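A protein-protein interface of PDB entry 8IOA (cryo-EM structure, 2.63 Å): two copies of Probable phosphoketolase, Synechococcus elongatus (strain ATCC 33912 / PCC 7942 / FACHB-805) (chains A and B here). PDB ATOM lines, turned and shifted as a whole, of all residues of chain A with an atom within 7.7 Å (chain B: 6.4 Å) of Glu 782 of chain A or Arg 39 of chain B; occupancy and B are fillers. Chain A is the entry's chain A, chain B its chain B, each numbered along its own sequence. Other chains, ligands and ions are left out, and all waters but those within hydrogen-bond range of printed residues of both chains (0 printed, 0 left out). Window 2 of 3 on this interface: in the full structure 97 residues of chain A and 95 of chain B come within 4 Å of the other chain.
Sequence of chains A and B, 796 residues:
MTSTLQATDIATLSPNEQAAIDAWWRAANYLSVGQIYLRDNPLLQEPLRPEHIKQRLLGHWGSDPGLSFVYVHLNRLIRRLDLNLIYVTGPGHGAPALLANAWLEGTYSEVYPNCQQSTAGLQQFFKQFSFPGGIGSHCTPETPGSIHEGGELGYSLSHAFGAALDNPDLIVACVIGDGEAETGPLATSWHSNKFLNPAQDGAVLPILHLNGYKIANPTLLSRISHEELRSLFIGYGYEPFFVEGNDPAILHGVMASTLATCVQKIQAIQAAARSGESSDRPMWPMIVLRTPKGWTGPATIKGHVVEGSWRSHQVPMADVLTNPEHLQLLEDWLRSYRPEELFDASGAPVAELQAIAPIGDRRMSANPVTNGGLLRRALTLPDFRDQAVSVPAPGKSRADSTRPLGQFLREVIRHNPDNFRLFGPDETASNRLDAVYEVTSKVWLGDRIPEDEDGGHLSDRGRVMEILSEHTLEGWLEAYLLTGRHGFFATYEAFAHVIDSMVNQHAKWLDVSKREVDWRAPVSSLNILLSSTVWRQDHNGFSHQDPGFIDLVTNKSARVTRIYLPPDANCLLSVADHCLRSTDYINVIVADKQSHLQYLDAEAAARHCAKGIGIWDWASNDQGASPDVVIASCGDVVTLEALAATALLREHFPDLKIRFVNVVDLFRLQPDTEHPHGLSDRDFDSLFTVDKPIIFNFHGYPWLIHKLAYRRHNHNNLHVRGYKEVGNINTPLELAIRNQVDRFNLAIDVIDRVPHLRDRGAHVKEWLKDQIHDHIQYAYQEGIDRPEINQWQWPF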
ATOM      1  N   THR A 731     -21.382 -11.375  10.310  1.00  0.00           N
ATOM      2  CA  THR A 731     -22.572 -11.967   9.730  1.00  0.00           C
ATOM      3  C   THR A 731     -22.378 -13.472   9.590  1.00  0.00           C
ATOM      4  O   THR A 731     -21.250 -13.965   9.626  1.00  0.00           O
ATOM      5  CB  THR A 731     -22.862 -11.344   8.369  1.00  0.00           C
ATOM      6  OG1 THR A 731     -21.860 -11.751   7.433  1.00  0.00           O
ATOM      7  CG2 THR A 731     -22.861  -9.835   8.469  1.00  0.00           C
ATOM      8  N   ILE A 776     -18.134  -9.826   1.205  1.00  0.00           N
ATOM      9  CA  ILE A 776     -17.563  -9.181   2.383  1.00  0.00           C
ATOM     10  C   ILE A 776     -17.809  -7.679   2.343  1.00  0.00           C
ATOM     11  O   ILE A 776     -18.168  -7.068   3.356  1.00  0.00           O
ATOM     12  CB  ILE A 776     -16.065  -9.507   2.500  1.00  0.00           C
ATOM     13  CG1 ILE A 776     -15.873 -10.973   2.877  1.00  0.00           C
ATOM     14  CG2 ILE A 776     -15.408  -8.618   3.529  1.00  0.00           C
ATOM     15  CD1 ILE A 776     -14.428 -11.367   3.037  1.00  0.00           C
ATOM     16  N   GLN A 777     -17.621  -7.059   1.178  1.00  0.00           N
ATOM     17  CA  GLN A 777     -17.851  -5.622   1.065  1.00  0.00           C
ATOM     18  C   GLN A 777     -19.305  -5.272   1.344  1.00  0.00           C
ATOM     19  O   GLN A 777     -19.592  -4.277   2.018  1.00  0.00           O
ATOM     20  CB  GLN A 777     -17.439  -5.127  -0.318  1.00  0.00           C
ATOM     21  CG  GLN A 777     -15.951  -5.191  -0.562  1.00  0.00           C
ATOM     22  CD  GLN A 777     -15.171  -4.375   0.443  1.00  0.00           C
ATOM     23  OE1 GLN A 777     -15.554  -3.255   0.778  1.00  0.00           O
ATOM     24  NE2 GLN A 777     -14.072  -4.934   0.934  1.00  0.00           N
ATOM     25  N   TYR A 778     -20.237  -6.070   0.827  1.00  0.00           N
ATOM     26  CA  TYR A 778     -21.648  -5.814   1.091  1.00  0.00           C
ATOM     27  C   TYR A 778     -21.962  -5.951   2.572  1.00  0.00           C
ATOM     28  O   TYR A 778     -22.768  -5.190   3.116  1.00  0.00           O
ATOM     29  CB  TYR A 778     -22.518  -6.761   0.270  1.00  0.00           C
ATOM     30  CG  TYR A 778     -23.996  -6.506   0.412  1.00  0.00           C
ATOM     31  CD1 TYR A 778     -24.635  -5.564  -0.377  1.00  0.00           C
ATOM     32  CD2 TYR A 778     -24.754  -7.212   1.330  1.00  0.00           C
ATOM     33  CE1 TYR A 778     -25.985  -5.332  -0.253  1.00  0.00           C
ATOM     34  CE2 TYR A 778     -26.104  -6.987   1.461  1.00  0.00           C
ATOM     35  CZ  TYR A 778     -26.714  -6.047   0.668  1.00  0.00           C
ATOM     36  OH  TYR A 778     -28.063  -5.819   0.797  1.00  0.00           O
ATOM     37  N   ALA A 779     -21.340  -6.924   3.240  1.00  0.00           N
ATOM     38  CA  ALA A 779     -21.582  -7.106   4.665  1.00  0.00           C
ATOM     39  C   ALA A 779     -21.142  -5.884   5.457  1.00  0.00           C
ATOM     40  O   ALA A 779     -21.822  -5.470   6.401  1.00  0.00           O
ATOM     41  CB  ALA A 779     -20.862  -8.355   5.166  1.00  0.00           C
ATOM     42  N   TYR A 780     -20.003  -5.298   5.096  1.00  0.00           N
ATOM     43  CA  TYR A 780     -19.521  -4.126   5.817  1.00  0.00           C
ATOM     44  C   TYR A 780     -20.421  -2.920   5.587  1.00  0.00           C
ATOM     45  O   TYR A 780     -20.625  -2.112   6.498  1.00  0.00           O
ATOM     46  CB  TYR A 780     -18.084  -3.818   5.409  1.00  0.00           C
ATOM     47  CG  TYR A 780     -17.065  -4.619   6.178  1.00  0.00           C
ATOM     48  CD1 TYR A 780     -17.160  -5.998   6.264  1.00  0.00           C
ATOM     49  CD2 TYR A 780     -16.008  -3.997   6.819  1.00  0.00           C
ATOM     50  CE1 TYR A 780     -16.235  -6.735   6.968  1.00  0.00           C
ATOM     51  CE2 TYR A 780     -15.076  -4.725   7.526  1.00  0.00           C
ATOM     52  CZ  TYR A 780     -15.195  -6.094   7.597  1.00  0.00           C
ATOM     53  OH  TYR A 780     -14.268  -6.825   8.300  1.00  0.00           O
ATOM     54  N   GLN A 781     -20.958  -2.772   4.377  1.00  0.00           N
ATOM     55  CA  GLN A 781     -21.804  -1.618   4.089  1.00  0.00           C
ATOM     56  C   GLN A 781     -23.186  -1.763   4.712  1.00  0.00           C
ATOM     57  O   GLN A 781     -23.740  -0.791   5.236  1.00  0.00           O
ATOM     58  CB  GLN A 781     -21.920  -1.417   2.581  1.00  0.00           C
ATOM     59  CG  GLN A 781     -20.599  -1.138   1.894  1.00  0.00           C
ATOM     60  CD  GLN A 781     -20.732  -1.092   0.389  1.00  0.00           C
ATOM     61  OE1 GLN A 781     -21.828  -1.231  -0.152  1.00  0.00           O
ATOM     62  NE2 GLN A 781     -19.613  -0.900  -0.299  1.00  0.00           N
ATOM     63  N   GLU A 782     -23.763  -2.965   4.665  1.00  0.00           N
ATOM     64  CA  GLU A 782     -25.140  -3.164   5.094  1.00  0.00           C
ATOM     65  C   GLU A 782     -25.283  -3.894   6.418  1.00  0.00           C
ATOM     66  O   GLU A 782     -26.329  -3.767   7.059  1.00  0.00           O
ATOM     67  CB  GLU A 782     -25.921  -3.938   4.024  1.00  0.00           C
ATOM     68  CG  GLU A 782     -26.051  -3.203   2.708  1.00  0.00           C
ATOM     69  CD  GLU A 782     -26.935  -1.980   2.813  1.00  0.00           C
ATOM     70  OE1 GLU A 782     -27.782  -1.936   3.729  1.00  0.00           O
ATOM     71  OE2 GLU A 782     -26.784  -1.060   1.982  1.00  0.00           O
ATOM     72  N   GLY A 783     -24.279  -4.653   6.843  1.00  0.00           N
ATOM     73  CA  GLY A 783     -24.376  -5.392   8.079  1.00  0.00           C
ATOM     74  C   GLY A 783     -25.138  -6.691   7.990  1.00  0.00           C
ATOM     75  O   GLY A 783     -25.275  -7.379   9.008  1.00  0.00           O
ATOM     76  N   ILE A 784     -25.640  -7.053   6.809  1.00  0.00           N
ATOM     77  CA  ILE A 784     -26.396  -8.282   6.616  1.00  0.00           C
ATOM     78  C   ILE A 784     -25.935  -8.935   5.319  1.00  0.00           C
ATOM     79  O   ILE A 784     -25.363  -8.289   4.440  1.00  0.00           O
ATOM     80  CB  ILE A 784     -27.920  -8.025   6.584  1.00  0.00           C
ATOM     81  CG1 ILE A 784     -28.694  -9.311   6.866  1.00  0.00           C
ATOM     82  CG2 ILE A 784     -28.337  -7.442   5.248  1.00  0.00           C
ATOM     83  CD1 ILE A 784     -28.384  -9.921   8.210  1.00  0.00           C
ATOM     84  N   ASP A 785     -26.181 -10.237   5.214  1.00  0.00           N
ATOM     85  CA  ASP A 785     -25.864 -10.956   3.992  1.00  0.00           C
ATOM     86  C   ASP A 785     -26.847 -10.592   2.885  1.00  0.00           C
ATOM     87  O   ASP A 785     -27.939 -10.072   3.130  1.00  0.00           O
ATOM     88  CB  ASP A 785     -25.896 -12.464   4.233  1.00  0.00           C
ATOM     89  CG  ASP A 785     -24.926 -12.902   5.307  1.00  0.00           C
ATOM     90  OD1 ASP A 785     -23.858 -12.271   5.434  1.00  0.00           O
ATOM     91  OD2 ASP A 785     -25.233 -13.877   6.025  1.00  0.00           O
ATOM     92  N   ARG A 786     -26.448 -10.874   1.649  1.00  0.00           N
ATOM     93  CA  ARG A 786     -27.322 -10.625   0.519  1.00  0.00           C
ATOM     94  C   ARG A 786     -28.546 -11.536   0.588  1.00  0.00           C
ATOM     95  O   ARG A 786     -28.483 -12.633   1.146  1.00  0.00           O
ATOM     96  CB  ARG A 786     -26.584 -10.857  -0.794  1.00  0.00           C
ATOM     97  CG  ARG A 786     -25.495  -9.850  -1.089  1.00  0.00           C
ATOM     98  CD  ARG A 786     -24.891 -10.109  -2.456  1.00  0.00           C
ATOM     99  NE  ARG A 786     -23.920  -9.092  -2.836  1.00  0.00           N
ATOM    100  CZ  ARG A 786     -24.229  -7.945  -3.424  1.00  0.00           C
ATOM    101  NH1 ARG A 786     -25.483  -7.626  -3.698  1.00  0.00           N
ATOM    102  NH2 ARG A 786     -23.257  -7.097  -3.744  1.00  0.00           N
ATOM    103  N   GLY B  34     -30.091   4.528  20.641  1.00  0.00           N
ATOM    104  CA  GLY B  34     -29.596   4.816  19.307  1.00  0.00           C
ATOM    105  C   GLY B  34     -28.625   3.769  18.803  1.00  0.00           C
ATOM    106  O   GLY B  34     -28.698   3.349  17.648  1.00  0.00           O
ATOM    107  N   TYR B  37     -30.505   0.525  17.728  1.00  0.00           N
ATOM    108  CA  TYR B  37     -31.401   0.622  16.585  1.00  0.00           C
ATOM    109  C   TYR B  37     -30.836   1.455  15.443  1.00  0.00           C
ATOM    110  O   TYR B  37     -30.701   0.955  14.325  1.00  0.00           O
ATOM    111  CB  TYR B  37     -32.747   1.196  17.034  1.00  0.00           C
ATOM    112  CG  TYR B  37     -33.561   0.239  17.860  1.00  0.00           C
ATOM    113  CD1 TYR B  37     -34.391  -0.688  17.257  1.00  0.00           C
ATOM    114  CD2 TYR B  37     -33.499   0.258  19.241  1.00  0.00           C
ATOM    115  CE1 TYR B  37     -35.136  -1.567  18.004  1.00  0.00           C
ATOM    116  CE2 TYR B  37     -34.241  -0.617  19.997  1.00  0.00           C
ATOM    117  CZ  TYR B  37     -35.057  -1.527  19.373  1.00  0.00           C
ATOM    118  OH  TYR B  37     -35.802  -2.405  20.121  1.00  0.00           O
ATOM    119  N   LEU B  38     -30.501   2.716  15.688  1.00  0.00           N
ATOM    120  CA  LEU B  38     -30.252   3.639  14.592  1.00  0.00           C
ATOM    121  C   LEU B  38     -28.959   3.311  13.861  1.00  0.00           C
ATOM    122  O   LEU B  38     -28.026   2.731  14.419  1.00  0.00           O
ATOM    123  CB  LEU B  38     -30.200   5.075  15.103  1.00  0.00           C
ATOM    124  CG  LEU B  38     -31.512   5.598  15.674  1.00  0.00           C
ATOM    125  CD1 LEU B  38     -31.418   7.085  15.913  1.00  0.00           C
ATOM    126  CD2 LEU B  38     -32.649   5.277  14.735  1.00  0.00           C
ATOM    127  N   ARG B  39     -28.918   3.698  12.589  1.00  0.00           N
ATOM    128  CA  ARG B  39     -27.742   3.554  11.742  1.00  0.00           C
ATOM    129  C   ARG B  39     -27.424   4.898  11.106  1.00  0.00           C
ATOM    130  O   ARG B  39     -26.279   5.170  10.736  1.00  0.00           O
ATOM    131  CB  ARG B  39     -27.980   2.484  10.676  1.00  0.00           C
ATOM    132  CG  ARG B  39     -26.879   2.357   9.653  1.00  0.00           C
ATOM    133  CD  ARG B  39     -27.146   1.221   8.685  1.00  0.00           C
ATOM    134  NE  ARG B  39     -28.377   1.417   7.930  1.00  0.00           N
ATOM    135  CZ  ARG B  39     -28.822   0.584   6.999  1.00  0.00           C
ATOM    136  NH1 ARG B  39     -28.156  -0.512   6.678  1.00  0.00           N
ATOM    137  NH2 ARG B  39     -29.963   0.859   6.376  1.00  0.00           N
ATOM    138  N   ASP B  40     -28.440   5.746  10.984  1.00  0.00           N
ATOM    139  CA  ASP B  40     -28.288   7.098  10.474  1.00  0.00           C
ATOM    140  C   ASP B  40     -29.271   7.994  11.214  1.00  0.00           C
ATOM    141  O   ASP B  40     -30.054   7.527  12.045  1.00  0.00           O
ATOM    142  CB  ASP B  40     -28.512   7.140   8.960  1.00  0.00           C
ATOM    143  CG  ASP B  40     -27.386   6.489   8.187  1.00  0.00           C
ATOM    144  OD1 ASP B  40     -26.312   6.260   8.778  1.00  0.00           O
ATOM    145  OD2 ASP B  40     -27.574   6.203   6.986  1.00  0.00           O
ATOM    146  N   ASN B  41     -29.230   9.287  10.913  1.00  0.00           N
ATOM    147  CA  ASN B  41     -30.139  10.264  11.500  1.00  0.00           C
ATOM    148  C   ASN B  41     -30.113  10.197  13.028  1.00  0.00           C
ATOM    149  O   ASN B  41     -31.135   9.898  13.660  1.00  0.00           O
ATOM    150  CB  ASN B  41     -31.553  10.063  10.974  1.00  0.00           C
ATOM    151  CG  ASN B  41     -32.494  11.164  11.397  1.00  0.00           C
ATOM    152  OD1 ASN B  41     -32.067  12.274  11.705  1.00  0.00           O
ATOM    153  ND2 ASN B  41     -33.785  10.865  11.417  1.00  0.00           N
ATOM    154  N   PRO B  42     -28.964  10.457  13.652  1.00  0.00           N
ATOM    155  CA  PRO B  42     -28.863  10.242  15.103  1.00  0.00           C
ATOM    156  C   PRO B  42     -29.777  11.129  15.927  1.00  0.00           C
ATOM    157  O   PRO B  42     -30.307  10.675  16.947  1.00  0.00           O
ATOM    158  CB  PRO B  42     -27.385  10.528  15.386  1.00  0.00           C
ATOM    159  CG  PRO B  42     -26.992  11.480  14.325  1.00  0.00           C
ATOM    160  CD  PRO B  42     -27.739  11.057  13.100  1.00  0.00           C
ATOM    161  N   PRO B  50     -37.257   3.631   7.378  1.00  0.00           N
ATOM    162  CA  PRO B  50     -36.666   2.292   7.526  1.00  0.00           C
ATOM    163  C   PRO B  50     -35.215   2.195   7.094  1.00  0.00           C
ATOM    164  O   PRO B  50     -34.538   1.240   7.489  1.00  0.00           O
ATOM    165  CB  PRO B  50     -37.565   1.415   6.647  1.00  0.00           C
ATOM    166  CG  PRO B  50     -38.856   2.136   6.609  1.00  0.00           C
ATOM    167  CD  PRO B  50     -38.505   3.589   6.600  1.00  0.00           C
ATOM    168  N   GLU B  51     -34.709   3.130   6.294  1.00  0.00           N
ATOM    169  CA  GLU B  51     -33.308   3.063   5.903  1.00  0.00           C
ATOM    170  C   GLU B  51     -32.363   3.530   7.000  1.00  0.00           C
ATOM    171  O   GLU B  51     -31.147   3.386   6.846  1.00  0.00           O
ATOM    172  CB  GLU B  51     -33.059   3.883   4.636  1.00  0.00           C
ATOM    173  CG  GLU B  51     -33.722   3.340   3.391  1.00  0.00           C
ATOM    174  CD  GLU B  51     -33.505   4.225   2.185  1.00  0.00           C
ATOM    175  OE1 GLU B  51     -33.000   5.354   2.355  1.00  0.00           O
ATOM    176  OE2 GLU B  51     -33.846   3.795   1.064  1.00  0.00           O
ATOM    177  N   HIS B  52     -32.886   4.087   8.093  1.00  0.00           N
ATOM    178  CA  HIS B  52     -32.056   4.512   9.211  1.00  0.00           C
ATOM    179  C   HIS B  52     -31.835   3.418  10.243  1.00  0.00           C
ATOM    180  O   HIS B  52     -30.948   3.558  11.089  1.00  0.00           O
ATOM    181  CB  HIS B  52     -32.684   5.719   9.909  1.00  0.00           C
ATOM    182  CG  HIS B  52     -32.913   6.892   9.010  1.00  0.00           C
ATOM    183  ND1 HIS B  52     -32.003   7.287   8.054  1.00  0.00           N
ATOM    184  CD2 HIS B  52     -33.949   7.759   8.923  1.00  0.00           C
ATOM    185  CE1 HIS B  52     -32.468   8.348   7.420  1.00  0.00           C
ATOM    186  NE2 HIS B  52     -33.647   8.654   7.929  1.00  0.00           N
ATOM    187  N   ILE B  53     -32.607   2.350  10.200  1.00  0.00           N
ATOM    188  CA  ILE B  53     -32.572   1.314  11.224  1.00  0.00           C
ATOM    189  C   ILE B  53     -31.653   0.188  10.772  1.00  0.00           C
ATOM    190  O   ILE B  53     -31.626  -0.173   9.592  1.00  0.00           O
ATOM    191  CB  ILE B  53     -33.992   0.796  11.521  1.00  0.00           C
ATOM    192  CG1 ILE B  53     -34.764   1.796  12.379  1.00  0.00           C
ATOM    193  CG2 ILE B  53     -33.949  -0.544  12.219  1.00  0.00           C
ATOM    194  CD1 ILE B  53     -35.351   2.948  11.614  1.00  0.00           C
ATOM    195  N   LYS B  54     -30.907  -0.382  11.713  1.00  0.00           N
ATOM    196  CA  LYS B  54     -30.005  -1.484  11.399  1.00  0.00           C
ATOM    197  C   LYS B  54     -30.822  -2.702  10.976  1.00  0.00           C
ATOM    198  O   LYS B  54     -31.883  -2.968  11.539  1.00  0.00           O
ATOM    199  CB  LYS B  54     -29.131  -1.826  12.607  1.00  0.00           C
ATOM    200  CG  LYS B  54     -27.991  -0.848  12.844  1.00  0.00           C
ATOM    201  CD  LYS B  54     -27.133  -1.277  14.022  1.00  0.00           C
ATOM    202  CE  LYS B  54     -26.032  -0.266  14.300  1.00  0.00           C
ATOM    203  NZ  LYS B  54     -26.400   0.670  15.398  1.00  0.00           N
ATOM    204  N   GLN B  55     -30.328  -3.440   9.987  1.00  0.00           N
ATOM    205  CA  GLN B  55     -31.039  -4.617   9.500  1.00  0.00           C
ATOM    206  C   GLN B  55     -31.075  -5.715  10.554  1.00  0.00           C
ATOM    207  O   GLN B  55     -32.133  -6.291  10.829  1.00  0.00           O
ATOM    208  CB  GLN B  55     -30.395  -5.131   8.214  1.00  0.00           C
ATOM    209  CG  GLN B  55     -30.795  -4.371   6.959  1.00  0.00           C
ATOM    210  CD  GLN B  55     -30.201  -2.981   6.901  1.00  0.00           C
ATOM    211  OE1 GLN B  55     -29.349  -2.621   7.712  1.00  0.00           O
ATOM    212  NE2 GLN B  55     -30.647  -2.189   5.935  1.00  0.00           N
ATOM    213  N   ARG B  56     -29.932  -6.017  11.158  1.00  0.00           N
ATOM    214  CA  ARG B  56     -29.825  -7.066  12.162  1.00  0.00           C
ATOM    215  C   ARG B  56     -29.587  -6.421  13.519  1.00  0.00           C
ATOM    216  O   ARG B  56     -28.583  -5.727  13.711  1.00  0.00           O
ATOM    217  CB  ARG B  56     -28.698  -8.038  11.815  1.00  0.00           C
ATOM    218  CG  ARG B  56     -28.701  -9.320  12.628  1.00  0.00           C
ATOM    219  CD  ARG B  56     -27.876 -10.395  11.939  1.00  0.00           C
ATOM    220  NE  ARG B  56     -26.490  -9.982  11.746  1.00  0.00           N
ATOM    221  CZ  ARG B  56     -25.466 -10.441  12.451  1.00  0.00           C
ATOM    222  NH1 ARG B  56     -25.632 -11.358  13.390  1.00  0.00           N
ATOM    223  NH2 ARG B  56     -24.247  -9.973  12.207  1.00  0.00           N
ATOM    224  N   GLN B 123     -23.467   9.785  14.276  1.00  0.00           N
ATOM    225  CA  GLN B 123     -23.823   8.853  13.214  1.00  0.00           C
ATOM    226  C   GLN B 123     -22.822   7.712  13.143  1.00  0.00           C
ATOM    227  O   GLN B 123     -23.204   6.547  12.995  1.00  0.00           O
ATOM    228  CB  GLN B 123     -23.907   9.594  11.880  1.00  0.00           C
ATOM    229  CG  GLN B 123     -24.515   8.792  10.744  1.00  0.00           C
ATOM    230  CD  GLN B 123     -23.517   7.872  10.073  1.00  0.00           C
ATOM    231  OE1 GLN B 123     -22.309   8.088  10.149  1.00  0.00           O
ATOM    232  NE2 GLN B 123     -24.018   6.837   9.413  1.00  0.00           N
ATOM    233  N   GLN B 124     -21.532   8.027  13.251  1.00  0.00           N
ATOM    234  CA  GLN B 124     -20.519   6.983  13.313  1.00  0.00           C
ATOM    235  C   GLN B 124     -20.624   6.190  14.608  1.00  0.00           C
ATOM    236  O   GLN B 124     -20.408   4.974  14.619  1.00  0.00           O
ATOM    237  CB  GLN B 124     -19.130   7.598  13.168  1.00  0.00           C
ATOM    238  CG  GLN B 124     -17.998   6.596  13.239  1.00  0.00           C
ATOM    239  CD  GLN B 124     -17.999   5.635  12.071  1.00  0.00           C
ATOM    240  OE1 GLN B 124     -18.592   5.906  11.027  1.00  0.00           O
ATOM    241  NE2 GLN B 124     -17.331   4.501  12.240  1.00  0.00           N
ATOM    242  N   PHE B 126     -23.352   5.567  16.537  1.00  0.00           N
ATOM    243  CA  PHE B 126     -24.467   4.627  16.478  1.00  0.00           C
ATOM    244  C   PHE B 126     -24.195   3.508  15.484  1.00  0.00           C
ATOM    245  O   PHE B 126     -24.523   2.346  15.738  1.00  0.00           O
ATOM    246  CB  PHE B 126     -25.754   5.355  16.101  1.00  0.00           C
ATOM    247  CG  PHE B 126     -26.298   6.233  17.183  1.00  0.00           C
ATOM    248  CD1 PHE B 126     -25.798   6.169  18.463  1.00  0.00           C
ATOM    249  CD2 PHE B 126     -27.321   7.116  16.917  1.00  0.00           C
ATOM    250  CE1 PHE B 126     -26.303   6.974  19.453  1.00  0.00           C
ATOM    251  CE2 PHE B 126     -27.828   7.922  17.905  1.00  0.00           C
ATOM    252  CZ  PHE B 126     -27.319   7.851  19.173  1.00  0.00           C
ATOM    253  N   LYS B 127     -23.596   3.847  14.343  1.00  0.00           N
ATOM    254  CA  LYS B 127     -23.425   2.881  13.266  1.00  0.00           C
ATOM    255  C   LYS B 127     -22.537   1.720  13.689  1.00  0.00           C
ATOM    256  O   LYS B 127     -22.805   0.566  13.338  1.00  0.00           O
ATOM    257  CB  LYS B 127     -22.846   3.589  12.043  1.00  0.00           C
ATOM    258  CG  LYS B 127     -22.300   2.684  10.964  1.00  0.00           C
ATOM    259  CD  LYS B 127     -23.401   1.941  10.249  1.00  0.00           C
ATOM    260  CE  LYS B 127     -22.973   1.588   8.839  1.00  0.00           C
ATOM    261  NZ  LYS B 127     -21.604   1.008   8.814  1.00  0.00           N
ATOM    262  N   PHE B 131     -22.032  -4.124  14.795  1.00  0.00           N
ATOM    263  CA  PHE B 131     -22.028  -4.027  13.351  1.00  0.00           C
ATOM    264  C   PHE B 131     -20.742  -4.635  12.811  1.00  0.00           C
ATOM    265  O   PHE B 131     -19.687  -4.508  13.442  1.00  0.00           O
ATOM    266  CB  PHE B 131     -22.137  -2.560  12.923  1.00  0.00           C
ATOM    267  CG  PHE B 131     -22.604  -2.368  11.518  1.00  0.00           C
ATOM    268  CD1 PHE B 131     -23.951  -2.279  11.233  1.00  0.00           C
ATOM    269  CD2 PHE B 131     -21.697  -2.259  10.485  1.00  0.00           C
ATOM    270  CE1 PHE B 131     -24.383  -2.095   9.944  1.00  0.00           C
ATOM    271  CE2 PHE B 131     -22.125  -2.078   9.194  1.00  0.00           C
ATOM    272  CZ  PHE B 131     -23.470  -1.995   8.922  1.00  0.00           C
ATOM    273  N   PRO B 132     -20.794  -5.301  11.660  1.00  0.00           N
ATOM    274  CA  PRO B 132     -19.566  -5.856  11.082  1.00  0.00           C
ATOM    275  C   PRO B 132     -18.532  -4.765  10.856  1.00  0.00           C
ATOM    276  O   PRO B 132     -18.854  -3.654  10.433  1.00  0.00           O
ATOM    277  CB  PRO B 132     -20.043  -6.468   9.764  1.00  0.00           C
ATOM    278  CG  PRO B 132     -21.468  -6.797  10.015  1.00  0.00           C
ATOM    279  CD  PRO B 132     -21.990  -5.715  10.912  1.00  0.00           C
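OE1 of Glu 782 of chain A lies within salt-bridge range of NH1 of Arg 39 of chain B (3.3 Å). The backbone carbonyl oxygen of Glu 782 of chain A sits close to the side-chain amide oxygen of Gln 55 of chain B, 3.3 Å away.
The backbone carbonyl oxygen (O) of His 52 of chain B sits at hydrogen-bond distance from the backbone NH (N) of Arg 39 of chain B. NE2 of Gln 123 of chain B lies within hydrogen-bond range of O of Arg 39 of chain B (3.1 Å). OE1 of Gln 55 of chain B lies within hydrogen-bond range of NH1 of Arg 39 of chain B (2.6 Å). O of Glu 51 of chain B sits at hydrogen-bond distance from NH2 of Arg 39 of chain B, at 2.8 Å. The side-chain hydroxyl (OG1) of Thr 731 of chain A sits at hydrogen-bond distance from the side-chain carboxylate (OD1) of Asp 785 of chain A.
Arg 56 of chain B touches Thr 731 of chain A (NH2 to CA, 3.6 Å). Pro 132 of chain B touches Thr 731 of chain A. Ala 779 of chain A touches Pro 132 of chain B. O of Tyr 780 of chain A touches CE2 of Phe 131 of chain B (3.1 Å). Gln 781 of chain A touches Phe 131 of chain B (O to CZ, 3.9 Å). Phe 131 of chain B touches Glu 782 of chain A (CZ to C, 3.6 Å). Gly 783 of chain A touches Arg 56 of chain B (O to NE, 3.97 Å). Gly 783 of chain A touches Phe 131 of chain B. CA of Gly 783 of chain A touches CD of Pro 132 of chain B, 3.7 Å away. CD1 of Ile 784 of chain A touches CD of Arg 56 of chain B (3.8 Å).
Glu 782 of chain A touches three residues of chain B. Arg 39 of chain B touches one residue of chain A. Of the printed residues of chain B, Thr 731 of chain A touches Arg 56 (3.6 Å) and Pro 132 (3.7 Å). Printed residues of chain B within 4 Å of Gly 783 of chain A: Arg 56 (3.97 Å), Phe 131 (3.5 Å) and Pro 132 (3.7 Å). Of the printed residues of chain B, Ala 779 of chain A touches Pro 132 (3.9 Å). Arg 786 of chain A touches none of the printed residues of chain B. Pro 42 of chain B touches none of the printed residues of chain A.
Printed residues of chain B that touch a printed residue of chain A: Arg 39, Gln 55, Arg 56, Phe 131 and Pro 132. Of the 12 printed residues of chain A, 7 touch a printed residue of chain B. Among the printed residues, 12 pairs touch across the chains. Among the printed residues, Asp or Glu carboxylates within 4 Å of a Lys or Arg side-chain nitrogen of the other chain: Glu 782 of chain A with Arg 39 of chain B (3.3 Å).
No position is printed for both chains. Of the 12 pairs that touch across the chains among the printed residues, none has its exchanged pair printed and touching as well.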
